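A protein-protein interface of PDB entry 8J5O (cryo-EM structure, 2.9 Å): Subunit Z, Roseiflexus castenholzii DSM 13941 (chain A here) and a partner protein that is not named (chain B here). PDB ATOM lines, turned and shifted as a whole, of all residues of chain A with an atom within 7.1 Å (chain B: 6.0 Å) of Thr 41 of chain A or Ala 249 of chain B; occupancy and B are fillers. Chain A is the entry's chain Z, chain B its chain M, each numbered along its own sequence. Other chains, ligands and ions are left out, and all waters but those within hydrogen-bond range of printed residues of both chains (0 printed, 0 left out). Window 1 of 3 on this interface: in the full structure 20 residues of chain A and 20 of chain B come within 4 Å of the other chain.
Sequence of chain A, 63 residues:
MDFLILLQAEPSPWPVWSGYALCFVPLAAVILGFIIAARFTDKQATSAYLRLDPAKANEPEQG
O of Gln 44 of chain A is in hydrogen-bond range of OG of Ser 47 of chain A (2.6 Å). The backbone carbonyl oxygen (O) of Asp 42 of chain A sits at hydrogen-bond distance from the side-chain hydroxyl (OG1) of Thr 46 of chain A, at 3.0 Å. The side-chain amide oxygen (OD1) of Asn 250 of chain B is in hydrogen-bond range of the backbone NH (N) of Asn 253 of chain B, 3.4 Å away. O of Ala 37 of chain A lies within hydrogen-bond range of OG1 of Thr 41 of chain A (2.7 Å). The backbone carbonyl oxygen (O) of Ala 249 of chain B lies close to the side-chain amide oxygen (OE1) of Gln 238 of chain B.
Of the 10 printed residues of chain B, 7 touch a printed residue of chain A. Among the printed residues, 15 pairs touch across the chains.
The indole nitrogen of Trp 257 of chain B lies within hydrogen-bond range of the side-chain hydroxyl of Thr 41 of chain A (3.0 Å).
Among the printed residues, merely in contact across the chains: Thr 41 of chain A with Ala 249 of chain B, Ala 38 of chain A with Trp 247 of chain B, Thr 41 of chain A with Asn 253 of chain B, Ala 45 of chain A with Ala 249 of chain B, Asp 42 of chain A with Trp 247 of chain B, Tyr 49 of chain A with Gln 238 of chain B, Gln 44 of chain A with Asn 250 of chain B, Asp 42 of chain A with Asn 248 of chain B, Ala 37 of chain A with Trp 257 of chain B, Tyr 49 of chain A with Asn 250 of chain B, Ala 45 of chain A with Asn 248 of chain B, Ala 45 of chain A with Asn 250 of chain B, Ala 38 of chain A with Trp 257 of chain B and Gln 44 of chain A with Asn 253 of chain B.
Of chain B, only Ala 249 (3.3 Å), Asn 253 (3.5 Å) and Trp 257 (3.0 Å) come within 4 Å of Thr 41 of chain A. Printed residues of chain B within 4 Å of Ala 38 of chain A: Trp 247 (3.5 Å) and Trp 257 (3.9 Å). Printed residues of chain B within 4 Å of Ala 37 of chain A: Trp 257 (3.8 Å). Printed residues of chain A within 4 Å of Asn 248 of chain B: Asp 42 (3.8 Å) and Ala 45 (3.8 Å). Printed residues of chain B within 4 Å of Gln 44 of chain A: Asn 250 (3.7 Å) and Asn 253 (3.9 Å). Of the printed residues of chain B, Ala 45 of chain A touches Asn 248 (3.8 Å), Ala 249 (3.6 Å) and Asn 250 (3.8 Å). Ile 35 of chain A touches none of the printed residues of chain B. Ile 254 of chain B touches none of the printed residues of chain A. The nearest residue of chain B that does not touch Thr 41 of chain A is Asn 248 of chain B (4.1 Å).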
ATOM      1  N   ILE A  35      -4.915 -33.049 -18.259  1.00  0.00           N
ATOM      2  CA  ILE A  35      -5.485 -33.317 -19.580  1.00  0.00           C
ATOM      3  C   ILE A  35      -6.488 -32.230 -19.965  1.00  0.00           C
ATOM      4  O   ILE A  35      -6.476 -31.719 -21.093  1.00  0.00           O
ATOM      5  CB  ILE A  35      -6.121 -34.719 -19.620  1.00  0.00           C
ATOM      6  CG1 ILE A  35      -5.053 -35.790 -19.395  1.00  0.00           C
ATOM      7  CG2 ILE A  35      -6.833 -34.946 -20.944  1.00  0.00           C
ATOM      8  CD1 ILE A  35      -5.615 -37.172 -19.162  1.00  0.00           C
ATOM      9  N   ILE A  36      -7.357 -31.847 -19.025  1.00  0.00           N
ATOM     10  CA  ILE A  36      -8.375 -30.836 -19.309  1.00  0.00           C
ATOM     11  C   ILE A  36      -7.736 -29.481 -19.595  1.00  0.00           C
ATOM     12  O   ILE A  36      -8.129 -28.775 -20.537  1.00  0.00           O
ATOM     13  CB  ILE A  36      -9.373 -30.757 -18.140  1.00  0.00           C
ATOM     14  CG1 ILE A  36     -10.140 -32.073 -17.999  1.00  0.00           C
ATOM     15  CG2 ILE A  36     -10.322 -29.594 -18.322  1.00  0.00           C
ATOM     16  CD1 ILE A  36     -10.949 -32.173 -16.728  1.00  0.00           C
ATOM     17  N   ALA A  37      -6.754 -29.087 -18.777  1.00  0.00           N
ATOM     18  CA  ALA A  37      -6.094 -27.804 -18.976  1.00  0.00           C
ATOM     19  C   ALA A  37      -5.360 -27.767 -20.308  1.00  0.00           C
ATOM     20  O   ALA A  37      -5.390 -26.751 -21.009  1.00  0.00           O
ATOM     21  CB  ALA A  37      -5.135 -27.526 -17.820  1.00  0.00           C
ATOM     22  N   ALA A  38      -4.702 -28.870 -20.680  1.00  0.00           N
ATOM     23  CA  ALA A  38      -4.040 -28.927 -21.977  1.00  0.00           C
ATOM     24  C   ALA A  38      -5.045 -28.802 -23.113  1.00  0.00           C
ATOM     25  O   ALA A  38      -4.800 -28.091 -24.095  1.00  0.00           O
ATOM     26  CB  ALA A  38      -3.243 -30.224 -22.099  1.00  0.00           C
ATOM     27  N   ARG A  39      -6.193 -29.474 -22.990  1.00  0.00           N
ATOM     28  CA  ARG A  39      -7.190 -29.431 -24.053  1.00  0.00           C
ATOM     29  C   ARG A  39      -7.727 -28.015 -24.241  1.00  0.00           C
ATOM     30  O   ARG A  39      -7.838 -27.521 -25.370  1.00  0.00           O
ATOM     31  CB  ARG A  39      -8.321 -30.410 -23.734  1.00  0.00           C
ATOM     32  CG  ARG A  39      -9.365 -30.583 -24.822  1.00  0.00           C
ATOM     33  CD  ARG A  39     -10.552 -29.662 -24.668  1.00  0.00           C
ATOM     34  NE  ARG A  39     -11.536 -29.926 -25.712  1.00  0.00           N
ATOM     35  CZ  ARG A  39     -11.502 -29.400 -26.928  1.00  0.00           C
ATOM     36  NH1 ARG A  39     -10.543 -28.568 -27.297  1.00  0.00           N
ATOM     37  NH2 ARG A  39     -12.450 -29.727 -27.802  1.00  0.00           N
ATOM     38  N   PHE A  40      -8.031 -27.328 -23.138  1.00  0.00           N
ATOM     39  CA  PHE A  40      -8.588 -25.981 -23.258  1.00  0.00           C
ATOM     40  C   PHE A  40      -7.530 -24.963 -23.677  1.00  0.00           C
ATOM     41  O   PHE A  40      -7.832 -24.017 -24.418  1.00  0.00           O
ATOM     42  CB  PHE A  40      -9.272 -25.576 -21.955  1.00  0.00           C
ATOM     43  CG  PHE A  40     -10.584 -26.271 -21.733  1.00  0.00           C
ATOM     44  CD1 PHE A  40     -11.607 -26.141 -22.657  1.00  0.00           C
ATOM     45  CD2 PHE A  40     -10.796 -27.056 -20.617  1.00  0.00           C
ATOM     46  CE1 PHE A  40     -12.816 -26.778 -22.469  1.00  0.00           C
ATOM     47  CE2 PHE A  40     -12.007 -27.694 -20.424  1.00  0.00           C
ATOM     48  CZ  PHE A  40     -13.015 -27.554 -21.351  1.00  0.00           C
ATOM     49  N   THR A  41      -6.284 -25.143 -23.231  1.00  0.00           N
ATOM     50  CA  THR A  41      -5.201 -24.293 -23.712  1.00  0.00           C
ATOM     51  C   THR A  41      -5.029 -24.431 -25.218  1.00  0.00           C
ATOM     52  O   THR A  41      -4.874 -23.429 -25.926  1.00  0.00           O
ATOM     53  CB  THR A  41      -3.899 -24.639 -22.990  1.00  0.00           C
ATOM     54  OG1 THR A  41      -4.060 -24.433 -21.582  1.00  0.00           O
ATOM     55  CG2 THR A  41      -2.760 -23.777 -23.496  1.00  0.00           C
ATOM     56  N   ASP A  42      -5.069 -25.666 -25.728  1.00  0.00           N
ATOM     57  CA  ASP A  42      -4.941 -25.876 -27.166  1.00  0.00           C
ATOM     58  C   ASP A  42      -6.123 -25.266 -27.914  1.00  0.00           C
ATOM     59  O   ASP A  42      -5.946 -24.666 -28.982  1.00  0.00           O
ATOM     60  CB  ASP A  42      -4.818 -27.372 -27.462  1.00  0.00           C
ATOM     61  CG  ASP A  42      -4.464 -27.664 -28.912  1.00  0.00           C
ATOM     62  OD1 ASP A  42      -4.335 -26.718 -29.716  1.00  0.00           O
ATOM     63  OD2 ASP A  42      -4.322 -28.855 -29.251  1.00  0.00           O
ATOM     64  N   LYS A  43      -7.335 -25.407 -27.365  1.00  0.00           N
ATOM     65  CA  LYS A  43      -8.512 -24.808 -27.995  1.00  0.00           C
ATOM     66  C   LYS A  43      -8.370 -23.297 -28.115  1.00  0.00           C
ATOM     67  O   LYS A  43      -8.655 -22.719 -29.171  1.00  0.00           O
ATOM     68  CB  LYS A  43      -9.779 -25.144 -27.207  1.00  0.00           C
ATOM     69  CG  LYS A  43     -11.040 -24.638 -27.900  1.00  0.00           C
ATOM     70  CD  LYS A  43     -12.313 -24.892 -27.108  1.00  0.00           C
ATOM     71  CE  LYS A  43     -12.719 -26.341 -27.137  1.00  0.00           C
ATOM     72  NZ  LYS A  43     -14.025 -26.580 -26.467  1.00  0.00           N
ATOM     73  N   GLN A  44      -7.941 -22.636 -27.038  1.00  0.00           N
ATOM     74  CA  GLN A  44      -7.771 -21.187 -27.097  1.00  0.00           C
ATOM     75  C   GLN A  44      -6.646 -20.803 -28.050  1.00  0.00           C
ATOM     76  O   GLN A  44      -6.747 -19.803 -28.768  1.00  0.00           O
ATOM     77  CB  GLN A  44      -7.510 -20.624 -25.701  1.00  0.00           C
ATOM     78  CG  GLN A  44      -7.139 -19.148 -25.687  1.00  0.00           C
ATOM     79  CD  GLN A  44      -8.124 -18.287 -26.453  1.00  0.00           C
ATOM     80  OE1 GLN A  44      -9.324 -18.557 -26.465  1.00  0.00           O
ATOM     81  NE2 GLN A  44      -7.621 -17.244 -27.097  1.00  0.00           N
ATOM     82  N   ALA A  45      -5.563 -21.585 -28.068  1.00  0.00           N
ATOM     83  CA  ALA A  45      -4.420 -21.252 -28.913  1.00  0.00           C
ATOM     84  C   ALA A  45      -4.764 -21.350 -30.393  1.00  0.00           C
ATOM     85  O   ALA A  45      -4.354 -20.498 -31.189  1.00  0.00           O
ATOM     86  CB  ALA A  45      -3.241 -22.163 -28.577  1.00  0.00           C
ATOM     87  N   THR A  46      -5.512 -22.382 -30.787  1.00  0.00           N
ATOM     88  CA  THR A  46      -5.777 -22.602 -32.205  1.00  0.00           C
ATOM     89  C   THR A  46      -6.996 -21.846 -32.721  1.00  0.00           C
ATOM     90  O   THR A  46      -7.338 -21.994 -33.899  1.00  0.00           O
ATOM     91  CB  THR A  46      -5.949 -24.097 -32.487  1.00  0.00           C
ATOM     92  OG1 THR A  46      -7.065 -24.603 -31.747  1.00  0.00           O
ATOM     93  CG2 THR A  46      -4.697 -24.859 -32.097  1.00  0.00           C
ATOM     94  N   SER A  47      -7.654 -21.049 -31.885  1.00  0.00           N
ATOM     95  CA  SER A  47      -8.801 -20.276 -32.341  1.00  0.00           C
ATOM     96  C   SER A  47      -8.364 -19.194 -33.325  1.00  0.00           C
ATOM     97  O   SER A  47      -7.177 -19.011 -33.609  1.00  0.00           O
ATOM     98  CB  SER A  47      -9.526 -19.644 -31.155  1.00  0.00           C
ATOM     99  OG  SER A  47      -8.631 -18.889 -30.360  1.00  0.00           O
ATOM    100  N   TYR A  49      -8.145 -15.239 -34.247  1.00  0.00           N
ATOM    101  CA  TYR A  49      -8.104 -13.901 -33.670  1.00  0.00           C
ATOM    102  C   TYR A  49      -7.146 -13.053 -34.501  1.00  0.00           C
ATOM    103  O   TYR A  49      -6.680 -13.478 -35.563  1.00  0.00           O
ATOM    104  CB  TYR A  49      -7.727 -13.958 -32.184  1.00  0.00           C
ATOM    105  CG  TYR A  49      -6.520 -14.808 -31.847  1.00  0.00           C
ATOM    106  CD1 TYR A  49      -5.238 -14.404 -32.188  1.00  0.00           C
ATOM    107  CD2 TYR A  49      -6.666 -16.010 -31.172  1.00  0.00           C
ATOM    108  CE1 TYR A  49      -4.140 -15.176 -31.874  1.00  0.00           C
ATOM    109  CE2 TYR A  49      -5.574 -16.789 -30.857  1.00  0.00           C
ATOM    110  CZ  TYR A  49      -4.313 -16.367 -31.210  1.00  0.00           C
ATOM    111  OH  TYR A  49      -3.221 -17.140 -30.897  1.00  0.00           O
ATOM    112  N   GLN B 238       4.730 -21.153 -31.794  1.00  0.00           N
ATOM    113  CA  GLN B 238       3.559 -22.023 -31.777  1.00  0.00           C
ATOM    114  C   GLN B 238       3.728 -23.195 -32.732  1.00  0.00           C
ATOM    115  O   GLN B 238       3.413 -24.336 -32.384  1.00  0.00           O
ATOM    116  CB  GLN B 238       2.307 -21.225 -32.134  1.00  0.00           C
ATOM    117  CG  GLN B 238       1.917 -20.177 -31.110  1.00  0.00           C
ATOM    118  CD  GLN B 238       0.560 -19.573 -31.396  1.00  0.00           C
ATOM    119  OE1 GLN B 238      -0.064 -18.977 -30.520  1.00  0.00           O
ATOM    120  NE2 GLN B 238       0.094 -19.726 -32.625  1.00  0.00           N
ATOM    121  N   TRP B 241       6.332 -25.778 -31.250  1.00  0.00           N
ATOM    122  CA  TRP B 241       5.832 -26.621 -30.174  1.00  0.00           C
ATOM    123  C   TRP B 241       4.641 -27.470 -30.598  1.00  0.00           C
ATOM    124  O   TRP B 241       4.362 -28.483 -29.950  1.00  0.00           O
ATOM    125  CB  TRP B 241       5.489 -25.768 -28.955  1.00  0.00           C
ATOM    126  CG  TRP B 241       6.707 -25.452 -28.143  1.00  0.00           C
ATOM    127  CD1 TRP B 241       7.189 -24.219 -27.838  1.00  0.00           C
ATOM    128  CD2 TRP B 241       7.610 -26.394 -27.554  1.00  0.00           C
ATOM    129  NE1 TRP B 241       8.331 -24.329 -27.087  1.00  0.00           N
ATOM    130  CE2 TRP B 241       8.612 -25.655 -26.898  1.00  0.00           C
ATOM    131  CE3 TRP B 241       7.667 -27.791 -27.511  1.00  0.00           C
ATOM    132  CZ2 TRP B 241       9.657 -26.264 -26.207  1.00  0.00           C
ATOM    133  CZ3 TRP B 241       8.704 -28.392 -26.826  1.00  0.00           C
ATOM    134  CH2 TRP B 241       9.685 -27.630 -26.185  1.00  0.00           C
ATOM    135  N   TRP B 247       0.723 -30.246 -29.489  1.00  0.00           N
ATOM    136  CA  TRP B 247      -0.146 -29.207 -28.956  1.00  0.00           C
ATOM    137  C   TRP B 247       0.713 -28.063 -28.443  1.00  0.00           C
ATOM    138  O   TRP B 247       1.892 -28.240 -28.130  1.00  0.00           O
ATOM    139  CB  TRP B 247      -1.070 -29.748 -27.856  1.00  0.00           C
ATOM    140  CG  TRP B 247      -0.371 -30.097 -26.578  1.00  0.00           C
ATOM    141  CD1 TRP B 247       0.495 -31.130 -26.373  1.00  0.00           C
ATOM    142  CD2 TRP B 247      -0.483 -29.412 -25.326  1.00  0.00           C
ATOM    143  NE1 TRP B 247       0.931 -31.131 -25.072  1.00  0.00           N
ATOM    144  CE2 TRP B 247       0.345 -30.086 -24.408  1.00  0.00           C
ATOM    145  CE3 TRP B 247      -1.202 -28.296 -24.892  1.00  0.00           C
ATOM    146  CZ2 TRP B 247       0.473 -29.679 -23.084  1.00  0.00           C
ATOM    147  CZ3 TRP B 247      -1.073 -27.892 -23.579  1.00  0.00           C
ATOM    148  CH2 TRP B 247      -0.243 -28.584 -22.689  1.00  0.00           C
ATOM    149  N   ASN B 248       0.110 -26.882 -28.365  1.00  0.00           N
ATOM    150  CA  ASN B 248       0.849 -25.672 -28.026  1.00  0.00           C
ATOM    151  C   ASN B 248      -0.097 -24.704 -27.323  1.00  0.00           C
ATOM    152  O   ASN B 248      -1.255 -25.034 -27.049  1.00  0.00           O
ATOM    153  CB  ASN B 248       1.485 -25.069 -29.290  1.00  0.00           C
ATOM    154  CG  ASN B 248       0.458 -24.461 -30.225  1.00  0.00           C
ATOM    155  OD1 ASN B 248       0.258 -23.248 -30.243  1.00  0.00           O
ATOM    156  ND2 ASN B 248      -0.201 -25.304 -31.006  1.00  0.00           N
ATOM    157  N   ALA B 249       0.402 -23.504 -27.029  1.00  0.00           N
ATOM    158  CA  ALA B 249      -0.392 -22.442 -26.430  1.00  0.00           C
ATOM    159  C   ALA B 249      -0.062 -21.138 -27.141  1.00  0.00           C
ATOM    160  O   ALA B 249       0.694 -21.114 -28.114  1.00  0.00           O
ATOM    161  CB  ALA B 249      -0.131 -22.326 -24.926  1.00  0.00           C
ATOM    162  N   ASN B 250      -0.657 -20.050 -26.663  1.00  0.00           N
ATOM    163  CA  ASN B 250      -0.330 -18.723 -27.162  1.00  0.00           C
ATOM    164  C   ASN B 250       0.539 -17.995 -26.136  1.00  0.00           C
ATOM    165  O   ASN B 250       0.995 -18.576 -25.149  1.00  0.00           O
ATOM    166  CB  ASN B 250      -1.608 -17.972 -27.553  1.00  0.00           C
ATOM    167  CG  ASN B 250      -2.474 -17.579 -26.363  1.00  0.00           C
ATOM    168  OD1 ASN B 250      -2.021 -16.955 -25.406  1.00  0.00           O
ATOM    169  ND2 ASN B 250      -3.745 -17.945 -26.432  1.00  0.00           N
ATOM    170  N   SER B 251       0.779 -16.704 -26.361  1.00  0.00           N
ATOM    171  CA  SER B 251       1.640 -15.906 -25.500  1.00  0.00           C
ATOM    172  C   SER B 251       0.923 -15.392 -24.255  1.00  0.00           C
ATOM    173  O   SER B 251       1.388 -14.423 -23.643  1.00  0.00           O
ATOM    174  CB  SER B 251       2.228 -14.733 -26.285  1.00  0.00           C
ATOM    175  OG  SER B 251       1.217 -14.027 -26.983  1.00  0.00           O
ATOM    176  N   ASN B 253      -1.335 -17.928 -22.253  1.00  0.00           N
ATOM    177  CA  ASN B 253      -1.670 -19.074 -21.411  1.00  0.00           C
ATOM    178  C   ASN B 253      -0.464 -19.575 -20.621  1.00  0.00           C
ATOM    179  O   ASN B 253      -0.608 -20.095 -19.503  1.00  0.00           O
ATOM    180  CB  ASN B 253      -2.239 -20.198 -22.274  1.00  0.00           C
ATOM    181  CG  ASN B 253      -3.517 -19.804 -22.971  1.00  0.00           C
ATOM    182  OD1 ASN B 253      -4.224 -18.900 -22.529  1.00  0.00           O
ATOM    183  ND2 ASN B 253      -3.820 -20.477 -24.071  1.00  0.00           N
ATOM    184  N   ILE B 254       0.733 -19.440 -21.198  1.00  0.00           N
ATOM    185  CA  ILE B 254       1.940 -19.994 -20.587  1.00  0.00           C
ATOM    186  C   ILE B 254       2.203 -19.343 -19.234  1.00  0.00           C
ATOM    187  O   ILE B 254       2.702 -19.984 -18.298  1.00  0.00           O
ATOM    188  CB  ILE B 254       3.133 -19.838 -21.553  1.00  0.00           C
ATOM    189  CG1 ILE B 254       4.272 -20.791 -21.180  1.00  0.00           C
ATOM    190  CG2 ILE B 254       3.597 -18.392 -21.633  1.00  0.00           C
ATOM    191  CD1 ILE B 254       4.075 -22.195 -21.687  1.00  0.00           C
ATOM    192  N   TRP B 257       0.023 -20.949 -16.704  1.00  0.00           N
ATOM    193  CA  TRP B 257       0.602 -22.250 -16.376  1.00  0.00           C
ATOM    194  C   TRP B 257       1.726 -22.107 -15.354  1.00  0.00           C
ATOM    195  O   TRP B 257       1.774 -22.835 -14.351  1.00  0.00           O
ATOM    196  CB  TRP B 257       1.119 -22.914 -17.653  1.00  0.00           C
ATOM    197  CG  TRP B 257       0.085 -23.671 -18.443  1.00  0.00           C
ATOM    198  CD1 TRP B 257      -0.699 -23.175 -19.445  1.00  0.00           C
ATOM    199  CD2 TRP B 257      -0.248 -25.060 -18.330  1.00  0.00           C
ATOM    200  NE1 TRP B 257      -1.510 -24.161 -19.945  1.00  0.00           N
ATOM    201  CE2 TRP B 257      -1.253 -25.329 -19.277  1.00  0.00           C
ATOM    202  CE3 TRP B 257       0.198 -26.100 -17.510  1.00  0.00           C
ATOM    203  CZ2 TRP B 257      -1.818 -26.592 -19.429  1.00  0.00           C
ATOM    204  CZ3 TRP B 257      -0.363 -27.352 -17.661  1.00  0.00           C
ATOM    205  CH2 TRP B 257      -1.360 -27.589 -18.613  1.00  0.00           C
